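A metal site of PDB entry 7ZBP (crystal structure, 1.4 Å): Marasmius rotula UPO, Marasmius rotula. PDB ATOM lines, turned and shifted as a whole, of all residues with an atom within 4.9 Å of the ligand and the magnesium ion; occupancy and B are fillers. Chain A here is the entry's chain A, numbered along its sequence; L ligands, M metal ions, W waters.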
ATOM      1  N   PRO A  20       6.046  -9.866  19.933  1.00  0.00           N
ATOM      2  CA  PRO A  20       6.666  -8.889  20.841  1.00  0.00           C
ATOM      3  C   PRO A  20       5.658  -7.994  21.567  1.00  0.00           C
ATOM      4  O   PRO A  20       6.056  -7.099  22.296  1.00  0.00           O
ATOM      5  CB  PRO A  20       7.530  -8.096  19.894  1.00  0.00           C
ATOM      6  CG  PRO A  20       6.681  -8.035  18.624  1.00  0.00           C
ATOM      7  CD  PRO A  20       6.104  -9.416  18.525  1.00  0.00           C
ATOM      8  N   CYS A  21       4.367  -8.202  21.323  1.00  0.00           N
ATOM      9  CA  CYS A  21       3.296  -7.308  21.791  1.00  0.00           C
ATOM     10  C   CYS A  21       2.578  -7.996  22.947  1.00  0.00           C
ATOM     11  O   CYS A  21       1.893  -8.998  22.730  1.00  0.00           O
ATOM     12  CB  CYS A  21       2.280  -7.014  20.697  1.00  0.00           C
ATOM     13  SG  CYS A  21       0.898  -6.106  21.376  1.00  0.00           S
ATOM     14  N   PRO A  22       2.681  -7.487  24.190  1.00  0.00           N
ATOM     15  CA  PRO A  22       1.929  -8.091  25.280  1.00  0.00           C
ATOM     16  C   PRO A  22       0.409  -7.973  25.135  1.00  0.00           C
ATOM     17  O   PRO A  22      -0.337  -8.809  25.647  1.00  0.00           O
ATOM     18  CB  PRO A  22       2.398  -7.300  26.507  1.00  0.00           C
ATOM     19  CG  PRO A  22       2.834  -5.978  25.953  1.00  0.00           C
ATOM     20  CD  PRO A  22       3.437  -6.291  24.590  1.00  0.00           C
ATOM     21  N   GLY A  23      -0.043  -6.944  24.430  1.00  0.00           N
ATOM     22  CA  GLY A  23      -1.509  -6.741  24.258  1.00  0.00           C
ATOM     23  C   GLY A  23      -2.100  -7.866  23.437  1.00  0.00           C
ATOM     24  O   GLY A  23      -3.070  -8.493  23.897  1.00  0.00           O
ATOM     25  N   LEU A  24      -1.517  -8.166  22.297  1.00  0.00           N
ATOM     26  CA  LEU A  24      -2.050  -9.247  21.442  1.00  0.00           C
ATOM     27  C   LEU A  24      -1.726 -10.611  22.056  1.00  0.00           C
ATOM     28  O   LEU A  24      -2.553 -11.529  21.966  1.00  0.00           O
ATOM     29  CB  LEU A  24      -1.480  -9.146  20.036  1.00  0.00           C
ATOM     30  CG  LEU A  24      -1.785  -7.887  19.265  1.00  0.00           C
ATOM     31  CD1 LEU A  24      -1.098  -7.905  17.915  1.00  0.00           C
ATOM     32  CD2 LEU A  24      -3.287  -7.617  19.114  1.00  0.00           C
ATOM     33  N   LEU A  27      -4.401 -11.298  24.632  1.00  0.00           N
ATOM     34  CA  LEU A  27      -5.662 -11.682  23.997  1.00  0.00           C
ATOM     35  C   LEU A  27      -5.613 -13.120  23.523  1.00  0.00           C
ATOM     36  O   LEU A  27      -6.624 -13.818  23.703  1.00  0.00           O
ATOM     37  CB  LEU A  27      -5.993 -10.730  22.858  1.00  0.00           C
ATOM     38  CG  LEU A  27      -6.318  -9.308  23.259  1.00  0.00           C
ATOM     39  CD1 LEU A  27      -6.353  -8.393  22.047  1.00  0.00           C
ATOM     40  CD2 LEU A  27      -7.610  -9.220  24.057  1.00  0.00           C
ATOM     41  N   ILE A  45      -8.557  -8.858  15.204  1.00  0.00           N
ATOM     42  CA  ILE A  45      -7.868  -7.984  16.210  1.00  0.00           C
ATOM     43  C   ILE A  45      -8.877  -6.947  16.722  1.00  0.00           C
ATOM     44  O   ILE A  45      -8.959  -6.678  17.932  1.00  0.00           O
ATOM     45  CB  ILE A  45      -6.608  -7.343  15.639  1.00  0.00           C
ATOM     46  CG1 ILE A  45      -5.511  -8.393  15.413  1.00  0.00           C
ATOM     47  CG2 ILE A  45      -6.135  -6.203  16.541  1.00  0.00           C
ATOM     48  CD1 ILE A  45      -4.369  -7.914  14.554  1.00  0.00           C
ATOM     49  N   GLY A  49      -9.770  -6.873  20.608  1.00  0.00           N
ATOM     50  CA  GLY A  49      -9.387  -5.712  21.417  1.00  0.00           C
ATOM     51  C   GLY A  49     -10.606  -4.973  21.972  1.00  0.00           C
ATOM     52  O   GLY A  49     -10.534  -4.456  23.104  1.00  0.00           O
ATOM     53  N   TYR A  53     -10.508  -5.416  25.963  1.00  0.00           N
ATOM     54  CA  TYR A  53      -9.948  -4.175  26.546  1.00  0.00           C
ATOM     55  C   TYR A  53     -10.812  -2.937  26.416  1.00  0.00           C
ATOM     56  O   TYR A  53     -10.399  -1.893  26.917  1.00  0.00           O
ATOM     57  CB  TYR A  53      -8.600  -3.881  25.868  1.00  0.00           C
ATOM     58  CG  TYR A  53      -7.580  -4.997  25.925  1.00  0.00           C
ATOM     59  CD1 TYR A  53      -7.270  -5.632  27.106  1.00  0.00           C
ATOM     60  CD2 TYR A  53      -6.727  -5.219  24.874  1.00  0.00           C
ATOM     61  CE1 TYR A  53      -6.264  -6.570  27.168  1.00  0.00           C
ATOM     62  CE2 TYR A  53      -5.683  -6.120  24.941  1.00  0.00           C
ATOM     63  CZ  TYR A  53      -5.416  -6.798  26.097  1.00  0.00           C
ATOM     64  OH  TYR A  53      -4.413  -7.737  26.122  1.00  0.00           O
ATOM     65  N   VAL A  55     -10.897  -1.356  23.610  1.00  0.00           N
ATOM     66  CA  VAL A  55     -10.142  -0.571  22.627  1.00  0.00           C
ATOM     67  C   VAL A  55     -10.949  -0.554  21.333  1.00  0.00           C
ATOM     68  O   VAL A  55     -11.375  -1.615  20.892  1.00  0.00           O
ATOM     69  CB  VAL A  55      -8.717  -1.117  22.454  1.00  0.00           C
ATOM     70  CG1 VAL A  55      -7.972  -0.363  21.391  1.00  0.00           C
ATOM     71  CG2 VAL A  55      -7.944  -1.026  23.789  1.00  0.00           C
ATOM     72  N   LEU A  60      -7.140   0.084  16.398  1.00  0.00           N
ATOM     73  CA  LEU A  60      -6.763  -1.282  16.003  1.00  0.00           C
ATOM     74  C   LEU A  60      -6.709  -1.447  14.477  1.00  0.00           C
ATOM     75  O   LEU A  60      -5.920  -2.269  13.996  1.00  0.00           O
ATOM     76  CB  LEU A  60      -7.725  -2.242  16.667  1.00  0.00           C
ATOM     77  CG  LEU A  60      -7.662  -2.219  18.203  1.00  0.00           C
ATOM     78  CD1 LEU A  60      -8.716  -3.118  18.757  1.00  0.00           C
ATOM     79  CD2 LEU A  60      -6.301  -2.663  18.692  1.00  0.00           C
ATOM     80  N   ALA A  63      -3.195   0.382  13.585  1.00  0.00           N
ATOM     81  CA  ALA A  63      -2.066  -0.474  13.945  1.00  0.00           C
ATOM     82  C   ALA A  63      -2.131  -1.808  13.215  1.00  0.00           C
ATOM     83  O   ALA A  63      -1.092  -2.327  12.783  1.00  0.00           O
ATOM     84  CB  ALA A  63      -2.060  -0.682  15.439  1.00  0.00           C
ATOM     85  N   GLY A  64      -3.330  -2.389  13.156  1.00  0.00           N
ATOM     86  CA  GLY A  64      -3.479  -3.738  12.609  1.00  0.00           C
ATOM     87  C   GLY A  64      -3.014  -3.808  11.171  1.00  0.00           C
ATOM     88  O   GLY A  64      -2.328  -4.769  10.810  1.00  0.00           O
ATOM     89  N   GLY A  67       0.629  -3.837  10.991  1.00  0.00           N
ATOM     90  CA  GLY A  67       1.141  -5.155  11.368  1.00  0.00           C
ATOM     91  C   GLY A  67       1.004  -6.192  10.262  1.00  0.00           C
ATOM     92  O   GLY A  67       1.816  -7.118  10.146  1.00  0.00           O
ATOM     93  N   LEU A  82       5.157 -10.318  13.863  1.00  0.00           N
ATOM     94  CA  LEU A  82       5.239  -8.911  14.283  1.00  0.00           C
ATOM     95  C   LEU A  82       6.594  -8.567  14.863  1.00  0.00           C
ATOM     96  O   LEU A  82       6.858  -7.388  15.030  1.00  0.00           O
ATOM     97  CB  LEU A  82       4.143  -8.661  15.322  1.00  0.00           C
ATOM     98  CG  LEU A  82       2.714  -8.605  14.802  1.00  0.00           C
ATOM     99  CD1 LEU A  82       1.746  -8.558  15.971  1.00  0.00           C
ATOM    100  CD2 LEU A  82       2.469  -7.465  13.840  1.00  0.00           C
ATOM    101  N   ILE A  88       6.753  -2.246  12.854  1.00  0.00           N
ATOM    102  CA  ILE A  88       6.407  -1.671  14.172  1.00  0.00           C
ATOM    103  C   ILE A  88       7.532  -1.958  15.180  1.00  0.00           C
ATOM    104  O   ILE A  88       7.891  -1.008  15.900  1.00  0.00           O
ATOM    105  CB  ILE A  88       5.056  -2.222  14.662  1.00  0.00           C
ATOM    106  CG1 ILE A  88       3.916  -1.837  13.718  1.00  0.00           C
ATOM    107  CG2 ILE A  88       4.772  -1.751  16.066  1.00  0.00           C
ATOM    108  CD1 ILE A  88       2.608  -2.566  14.020  1.00  0.00           C
ATOM    109  N   GLU A  89       8.062  -3.175  15.213  1.00  0.00           N
ATOM    110  CA  GLU A  89       9.053  -3.581  16.221  1.00  0.00           C
ATOM    111  C   GLU A  89      10.214  -2.593  16.156  1.00  0.00           C
ATOM    112  O   GLU A  89      10.725  -2.279  15.059  1.00  0.00           O
ATOM    113  CB  GLU A  89       9.489  -5.039  16.051  1.00  0.00           C
ATOM    114  CG  GLU A  89      10.252  -5.576  17.264  1.00  0.00           C
ATOM    115  CD  GLU A  89      11.687  -5.122  17.343  1.00  0.00           C
ATOM    116  OE1 GLU A  89      12.306  -5.095  16.297  1.00  0.00           O
ATOM    117  OE2 GLU A  89      12.138  -4.809  18.476  1.00  0.00           O
ATOM    118  N   HIS A  90      10.690  -2.180  17.320  1.00  0.00           N
ATOM    119  CA  HIS A  90      11.692  -1.097  17.457  1.00  0.00           C
ATOM    120  C   HIS A  90      12.663  -1.428  18.595  1.00  0.00           C
ATOM    121  O   HIS A  90      12.384  -2.179  19.510  1.00  0.00           O
ATOM    122  CB  HIS A  90      10.985   0.255  17.695  1.00  0.00           C
ATOM    123  CG  HIS A  90      10.032   0.181  18.817  1.00  0.00           C
ATOM    124  ND1 HIS A  90      10.478   0.138  20.168  1.00  0.00           N
ATOM    125  CD2 HIS A  90       8.677   0.088  18.865  1.00  0.00           C
ATOM    126  CE1 HIS A  90       9.402  -0.031  20.939  1.00  0.00           C
ATOM    127  NE2 HIS A  90       8.277  -0.030  20.175  1.00  0.00           N
ATOM    128  N   ASP A  91      13.799  -0.778  18.532  1.00  0.00           N
ATOM    129  CA  ASP A  91      14.719  -0.731  19.675  1.00  0.00           C
ATOM    130  C   ASP A  91      14.113   0.037  20.834  1.00  0.00           C
ATOM    131  O   ASP A  91      13.120   0.791  20.720  1.00  0.00           O
ATOM    132  CB  ASP A  91      15.994  -0.052  19.204  1.00  0.00           C
ATOM    133  CG  ASP A  91      16.641  -0.777  18.033  1.00  0.00           C
ATOM    134  OD1 ASP A  91      16.515  -2.015  17.956  1.00  0.00           O
ATOM    135  OD2 ASP A  91      17.334  -0.064  17.264  1.00  0.00           O
ATOM    136  N   SER A  93      12.616  -1.129  23.533  1.00  0.00           N
ATOM    137  CA  SER A  93      11.383  -1.717  24.082  1.00  0.00           C
ATOM    138  C   SER A  93      11.419  -1.713  25.615  1.00  0.00           C
ATOM    139  O   SER A  93      12.533  -1.682  26.205  1.00  0.00           O
ATOM    140  CB  SER A  93      11.170  -3.134  23.573  1.00  0.00           C
ATOM    141  OG  SER A  93      10.915  -3.077  22.170  1.00  0.00           O
ATOM    142  N   LEU A  94      10.238  -1.839  26.214  1.00  0.00           N
ATOM    143  CA  LEU A  94      10.104  -1.866  27.690  1.00  0.00           C
ATOM    144  C   LEU A  94      10.492  -3.226  28.237  1.00  0.00           C
ATOM    145  O   LEU A  94      10.795  -3.328  29.444  1.00  0.00           O
ATOM    146  CB  LEU A  94       8.669  -1.551  28.040  1.00  0.00           C
ATOM    147  CG  LEU A  94       8.197  -0.173  27.589  1.00  0.00           C
ATOM    148  CD1 LEU A  94       6.702  -0.027  27.702  1.00  0.00           C
ATOM    149  CD2 LEU A  94       8.868   0.951  28.338  1.00  0.00           C
ATOM    150  N   SER A  95      10.319  -4.307  27.481  1.00  0.00           N
ATOM    151  CA  SER A  95      10.416  -5.666  28.015  1.00  0.00           C
ATOM    152  C   SER A  95      11.165  -6.623  27.103  1.00  0.00           C
ATOM    153  O   SER A  95      11.206  -7.820  27.461  1.00  0.00           O
ATOM    154  CB  SER A  95       9.066  -6.160  28.402  1.00  0.00           C
ATOM    155  OG  SER A  95       8.272  -6.413  27.229  1.00  0.00           O
ATOM    156  N   ARG A  96      11.695  -6.152  25.983  1.00  0.00           N
ATOM    157  CA  ARG A  96      12.420  -6.996  25.022  1.00  0.00           C
ATOM    158  C   ARG A  96      13.776  -6.349  24.788  1.00  0.00           C
ATOM    159  O   ARG A  96      13.922  -5.155  24.973  1.00  0.00           O
ATOM    160  CB  ARG A  96      11.662  -7.103  23.689  1.00  0.00           C
ATOM    161  CG  ARG A  96      10.612  -8.201  23.542  1.00  0.00           C
ATOM    162  CD  ARG A  96       9.467  -8.152  24.518  1.00  0.00           C
ATOM    163  NE  ARG A  96       8.481  -9.172  24.201  1.00  0.00           N
ATOM    164  CZ  ARG A  96       7.436  -9.448  24.956  1.00  0.00           C
ATOM    165  NH1 ARG A  96       7.171  -8.749  26.049  1.00  0.00           N
ATOM    166  NH2 ARG A  96       6.602 -10.400  24.579  1.00  0.00           N
ATOM    167  N   GLU A  97      14.732  -7.142  24.265  1.00  0.00           N
ATOM    168  CA  GLU A  97      16.054  -6.649  23.874  1.00  0.00           C
ATOM    169  C   GLU A  97      16.013  -6.108  22.458  1.00  0.00           C
ATOM    170  O   GLU A  97      15.135  -6.506  21.675  1.00  0.00           O
ATOM    171  CB  GLU A  97      17.095  -7.775  23.991  1.00  0.00           C
ATOM    172  CG  GLU A  97      17.214  -8.346  25.368  1.00  0.00           C
ATOM    173  CD  GLU A  97      18.111  -9.558  25.497  1.00  0.00           C
ATOM    174  OE1 GLU A  97      18.165 -10.364  24.569  1.00  0.00           O
ATOM    175  OE2 GLU A  97      18.819  -9.650  26.529  1.00  0.00           O
ATOM    176  N   ASN A 104      14.559  -9.859  20.321  1.00  0.00           N
ATOM    177  CA  ASN A 104      13.549  -8.783  20.208  1.00  0.00           C
ATOM    178  C   ASN A 104      12.111  -9.316  20.334  1.00  0.00           C
ATOM    179  O   ASN A 104      11.192  -8.524  20.117  1.00  0.00           O
ATOM    180  CB  ASN A 104      13.723  -7.981  18.926  1.00  0.00           C
ATOM    181  CG  ASN A 104      13.191  -8.695  17.708  1.00  0.00           C
ATOM    182  OD1 ASN A 104      13.062  -9.937  17.709  1.00  0.00           O
ATOM    183  ND2 ASN A 104      12.899  -7.947  16.660  1.00  0.00           N
ATOM    184  N   GLU A 161       2.599   2.855  22.878  1.00  0.00           N
ATOM    185  CA  GLU A 161       2.607   1.573  23.578  1.00  0.00           C
ATOM    186  C   GLU A 161       2.534   1.829  25.086  1.00  0.00           C
ATOM    187  O   GLU A 161       1.822   1.124  25.770  1.00  0.00           O
ATOM    188  CB  GLU A 161       3.845   0.756  23.158  1.00  0.00           C
ATOM    189  CG  GLU A 161       3.685   0.246  21.732  1.00  0.00           C
ATOM    190  CD  GLU A 161       4.931  -0.175  20.990  1.00  0.00           C
ATOM    191  OE1 GLU A 161       6.024   0.051  21.511  1.00  0.00           O
ATOM    192  OE2 GLU A 161       4.813  -0.620  19.836  1.00  0.00           O
ATOM    193  N   PHE A 164      -0.977   2.695  25.742  1.00  0.00           N
ATOM    194  CA  PHE A 164      -1.822   1.480  25.689  1.00  0.00           C
ATOM    195  C   PHE A 164      -1.801   0.803  27.050  1.00  0.00           C
ATOM    196  O   PHE A 164      -2.870   0.423  27.527  1.00  0.00           O
ATOM    197  CB  PHE A 164      -1.358   0.500  24.608  1.00  0.00           C
ATOM    198  CG  PHE A 164      -1.753   0.818  23.192  1.00  0.00           C
ATOM    199  CD1 PHE A 164      -2.225   2.064  22.825  1.00  0.00           C
ATOM    200  CD2 PHE A 164      -1.364  -0.028  22.176  1.00  0.00           C
ATOM    201  CE1 PHE A 164      -2.458   2.373  21.494  1.00  0.00           C
ATOM    202  CE2 PHE A 164      -1.646   0.259  20.852  1.00  0.00           C
ATOM    203  CZ  PHE A 164      -2.153   1.474  20.501  1.00  0.00           C
ATOM    204  N   PHE A 165      -0.646   0.496  27.630  1.00  0.00           N
ATOM    205  CA  PHE A 165      -0.674  -0.249  28.907  1.00  0.00           C
ATOM    206  C   PHE A 165      -1.268   0.624  30.019  1.00  0.00           C
ATOM    207  O   PHE A 165      -2.013   0.046  30.842  1.00  0.00           O
ATOM    208  CB  PHE A 165       0.682  -0.874  29.252  1.00  0.00           C
ATOM    209  CG  PHE A 165       1.700  -0.032  29.964  1.00  0.00           C
ATOM    210  CD1 PHE A 165       1.495   0.368  31.283  1.00  0.00           C
ATOM    211  CD2 PHE A 165       2.878   0.365  29.331  1.00  0.00           C
ATOM    212  CE1 PHE A 165       2.440   1.169  31.912  1.00  0.00           C
ATOM    213  CE2 PHE A 165       3.838   1.150  29.962  1.00  0.00           C
ATOM    214  CZ  PHE A 165       3.594   1.524  31.268  1.00  0.00           C
ATOM    215  N   VAL A 168      -5.270   0.515  29.142  1.00  0.00           N
ATOM    216  CA  VAL A 168      -5.971  -0.787  29.139  1.00  0.00           C
ATOM    217  C   VAL A 168      -5.912  -1.432  30.521  1.00  0.00           C
ATOM    218  O   VAL A 168      -6.879  -2.159  30.892  1.00  0.00           O
ATOM    219  CB  VAL A 168      -5.398  -1.679  28.037  1.00  0.00           C
ATOM    220  CG1 VAL A 168      -5.736  -3.115  28.192  1.00  0.00           C
ATOM    221  CG2 VAL A 168      -5.735  -1.124  26.648  1.00  0.00           C
ATOM    222  N   PHE A 187       0.395  -8.244  33.412  1.00  0.00           N
ATOM    223  CA  PHE A 187       0.217  -8.078  31.956  1.00  0.00           C
ATOM    224  C   PHE A 187       1.523  -8.396  31.238  1.00  0.00           C
ATOM    225  O   PHE A 187       1.544  -9.147  30.253  1.00  0.00           O
ATOM    226  CB  PHE A 187      -0.298  -6.666  31.723  1.00  0.00           C
ATOM    227  CG  PHE A 187      -0.518  -6.254  30.282  1.00  0.00           C
ATOM    228  CD1 PHE A 187      -1.503  -6.851  29.500  1.00  0.00           C
ATOM    229  CD2 PHE A 187       0.296  -5.309  29.728  1.00  0.00           C
ATOM    230  CE1 PHE A 187      -1.675  -6.428  28.183  1.00  0.00           C
ATOM    231  CE2 PHE A 187       0.115  -4.880  28.432  1.00  0.00           C
ATOM    232  CZ  PHE A 187      -0.866  -5.448  27.654  1.00  0.00           C
ATOM    233  N   PHE A 188       2.646  -7.805  31.638  1.00  0.00           N
ATOM    234  CA  PHE A 188       3.938  -8.013  30.976  1.00  0.00           C
ATOM    235  C   PHE A 188       4.491  -9.410  31.292  1.00  0.00           C
ATOM    236  O   PHE A 188       4.913 -10.107  30.386  1.00  0.00           O
ATOM    237  CB  PHE A 188       4.925  -6.916  31.350  1.00  0.00           C
ATOM    238  CG  PHE A 188       4.795  -5.645  30.549  1.00  0.00           C
ATOM    239  CD1 PHE A 188       5.499  -5.474  29.353  1.00  0.00           C
ATOM    240  CD2 PHE A 188       4.060  -4.570  31.019  1.00  0.00           C
ATOM    241  CE1 PHE A 188       5.425  -4.272  28.662  1.00  0.00           C
ATOM    242  CE2 PHE A 188       3.968  -3.393  30.306  1.00  0.00           C
ATOM    243  CZ  PHE A 188       4.650  -3.235  29.127  1.00  0.00           C
HETATM  244  C1  LIG L   1       4.465  -3.606  21.565  1.00  0.00           C
HETATM  245  C2  LIG L   1       0.324  -2.978  24.052  1.00  0.00           C
HETATM  246  C3  LIG L   1      -2.203  -3.804  19.975  1.00  0.00           C
HETATM  247  C4  LIG L   1       1.948  -4.581  17.559  1.00  0.00           C
HETATM  248  C5  LIG L   1       3.591  -3.271  22.543  1.00  0.00           C
HETATM  249  C6  LIG L   1       3.920  -2.837  23.853  1.00  0.00           C
HETATM  250  C7  LIG L   1       2.746  -2.632  24.550  1.00  0.00           C
HETATM  251  C8  LIG L   1       1.667  -2.982  23.674  1.00  0.00           C
HETATM  252  C9  LIG L   1       2.569  -2.170  26.016  1.00  0.00           C
HETATM  253  C10 LIG L   1       5.331  -2.548  24.296  1.00  0.00           C
HETATM  254  C11 LIG L   1       6.185  -3.732  24.659  1.00  0.00           C
HETATM  255  C12 LIG L   1       7.547  -3.366  25.050  1.00  0.00           C
HETATM  256  O1  LIG L   1       8.224  -4.299  25.601  1.00  0.00           O
HETATM  257  O2  LIG L   1       7.991  -2.253  24.811  1.00  0.00           O
HETATM  258  C13 LIG L   1      -0.723  -3.246  23.158  1.00  0.00           C
HETATM  259  C14 LIG L   1      -2.112  -3.205  23.538  1.00  0.00           C
HETATM  260  C15 LIG L   1      -2.796  -3.431  22.379  1.00  0.00           C
HETATM  261  C16 LIG L   1      -1.854  -3.618  21.281  1.00  0.00           C
HETATM  262  C17 LIG L   1      -2.730  -2.985  24.904  1.00  0.00           C
HETATM  263  C18 LIG L   1      -4.274  -3.570  22.289  1.00  0.00           C
HETATM  264  C19 LIG L   1      -4.793  -4.480  21.513  1.00  0.00           C
HETATM  265  C20 LIG L   1      -1.323  -3.960  18.956  1.00  0.00           C
HETATM  266  C21 LIG L   1      -1.647  -4.151  17.570  1.00  0.00           C
HETATM  267  C22 LIG L   1      -0.470  -4.380  16.866  1.00  0.00           C
HETATM  268  C23 LIG L   1       0.598  -4.382  17.870  1.00  0.00           C
HETATM  269  C24 LIG L   1      -3.064  -4.095  16.953  1.00  0.00           C
HETATM  270  C25 LIG L   1      -0.250  -4.763  15.462  1.00  0.00           C
HETATM  271  C26 LIG L   1      -1.121  -5.467  14.751  1.00  0.00           C
HETATM  272  C27 LIG L   1       2.975  -4.396  18.496  1.00  0.00           C
HETATM  273  C28 LIG L   1       4.374  -4.656  18.113  1.00  0.00           C
HETATM  274  C29 LIG L   1       5.075  -4.359  19.263  1.00  0.00           C
HETATM  275  C30 LIG L   1       4.080  -3.986  20.267  1.00  0.00           C
HETATM  276  C31 LIG L   1       4.971  -5.074  16.811  1.00  0.00           C
HETATM  277  C32 LIG L   1       6.571  -4.414  19.507  1.00  0.00           C
HETATM  278  C33 LIG L   1       7.165  -3.020  19.575  1.00  0.00           C
HETATM  279  C34 LIG L   1       8.463  -3.101  20.315  1.00  0.00           C
HETATM  280  O3  LIG L   1       9.566  -3.212  19.675  1.00  0.00           O
HETATM  281  O4  LIG L   1       8.387  -3.062  21.555  1.00  0.00           O
HETATM  282  N1  LIG L   1       2.189  -3.358  22.441  1.00  0.00           N
HETATM  283  N2  LIG L   1      -0.602  -3.461  21.829  1.00  0.00           N
HETATM  284  N3  LIG L   1       0.052  -4.019  19.083  1.00  0.00           N
HETATM  285  N4  LIG L   1       2.787  -4.064  19.780  1.00  0.00           N
HETATM  286 FE1  LIG L   1       1.130  -3.821  20.790  1.00  0.00          FE
HETATM  287 MG    MG M   1      11.484  -3.990  20.263  1.00  0.00          MG
HETATM  288  O   HOH W   1      10.581  -5.892  20.719  1.00  0.00           O
HETATM  289  O   HOH W   2       8.433  -5.769  22.478  1.00  0.00           O
HETATM  290  O   HOH W   3      13.295  -4.430  21.174  1.00  0.00           O
HETATM  291  O   HOH W   4       7.699   0.189  23.650  1.00  0.00           O
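The magnesium ion is bound by OE2 of Glu 89, water W3, O3 of the ligand, water W1, O of His 90 and OG of Ser 93.
The magnesium ion has six donor atoms within binding distance.
Water W4 lies within hydrogen-bond range of O2 of the ligand and OE1 of Glu 161.
Water W2 bridges the backbone carbonyl oxygen of Pro 20 and an oxygen (O4) of the ligand.
FE1 of the ligand is bound by SG of Cys 21 (2.4 Å).
The backbone NH (N) of Ser 95 sits at hydrogen-bond distance from an oxygen (O1) of the ligand, at 2.8 Å.
The backbone NH (N) of His 90 lies close to an oxygen (O3) of the ligand (2.8 Å).
The backbone NH (N) of Leu 94 is in hydrogen-bond range of an oxygen (O2) of the ligand (2.7 Å).
NE2 of His 90 lies close to O4 of the ligand.
The side-chain hydroxyl (OG) of Ser 95 lies within hydrogen-bond range of an oxygen (O1) of the ligand.
Residues that only touch the ligand: Pro 20 (3.7 Å), Pro 22 (3.6 Å), Gly 23 (3.7 Å), Leu 24 (3.7 Å), Ile 45 (3.7 Å), Tyr 53 (3.9 Å), Leu 60 (3.7 Å), Ala 63 (3.7 Å), Gly 64 (3.6 Å), Leu 82 (3.5 Å), Ile 88 (3.4 Å), Arg 96 (3.95 Å), Glu 161 (3.4 Å), Phe 164 (3.4 Å), Phe 165 (3.96 Å), Val 168 (3.9 Å) and Phe 188 (3.9 Å).
Hydrophobic or aromatic side chains within 4 Å of the ligand: Pro 20, Pro 22, Leu 24, Ile 45, Tyr 53, Leu 60, Ala 63, Leu 82, Ile 88, His 90, Leu 94, Phe 164, Phe 165, Val 168 and Phe 188.
Within 4 Å of the ligand: Pro 20, Cys 21, Pro 22, Gly 23, Leu 24, Ile 45, Tyr 53, Leu 60, Ala 63, Gly 64, Leu 82, Ile 88, Glu 89, His 90, Ser 93, Leu 94, Ser 95, Arg 96, Glu 161, Phe 164, Phe 165, Val 168 and Phe 188.
The nearest printed residue that does not touch the ligand is Gly 67 (4.1 Å).
The side-chain hydroxyl (OG) of Ser 95 is in hydrogen-bond range of the guanidinium group (NH1) of Arg 96, 2.8 Å away.
The side-chain sulfur (SG) of Cys 21 sits close to the backbone NH (N) of Leu 24 (3.3 Å).
The side-chain carboxylate (OE1) of Glu 89 is in hydrogen-bond range of the side-chain amide nitrogen (ND2) of Asn 104.
The side-chain sulfur of Cys 21 sits close to the backbone NH of Gly 23 (3.3 Å).
A ring nitrogen (NE2) of His 90 sits at hydrogen-bond distance from the side-chain carboxylate (OE1) of Glu 161, 2.6 Å away.
The side-chain hydroxyl (OH) of Tyr 53 sits at hydrogen-bond distance from the backbone carbonyl oxygen (O) of Gly 23, 2.7 Å away.
Within 4 Å of the magnesium ion: Glu 89, His 90 and Ser 93.
The nearest printed residue that does not touch the magnesium ion is Asp 91 (4.3 Å).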
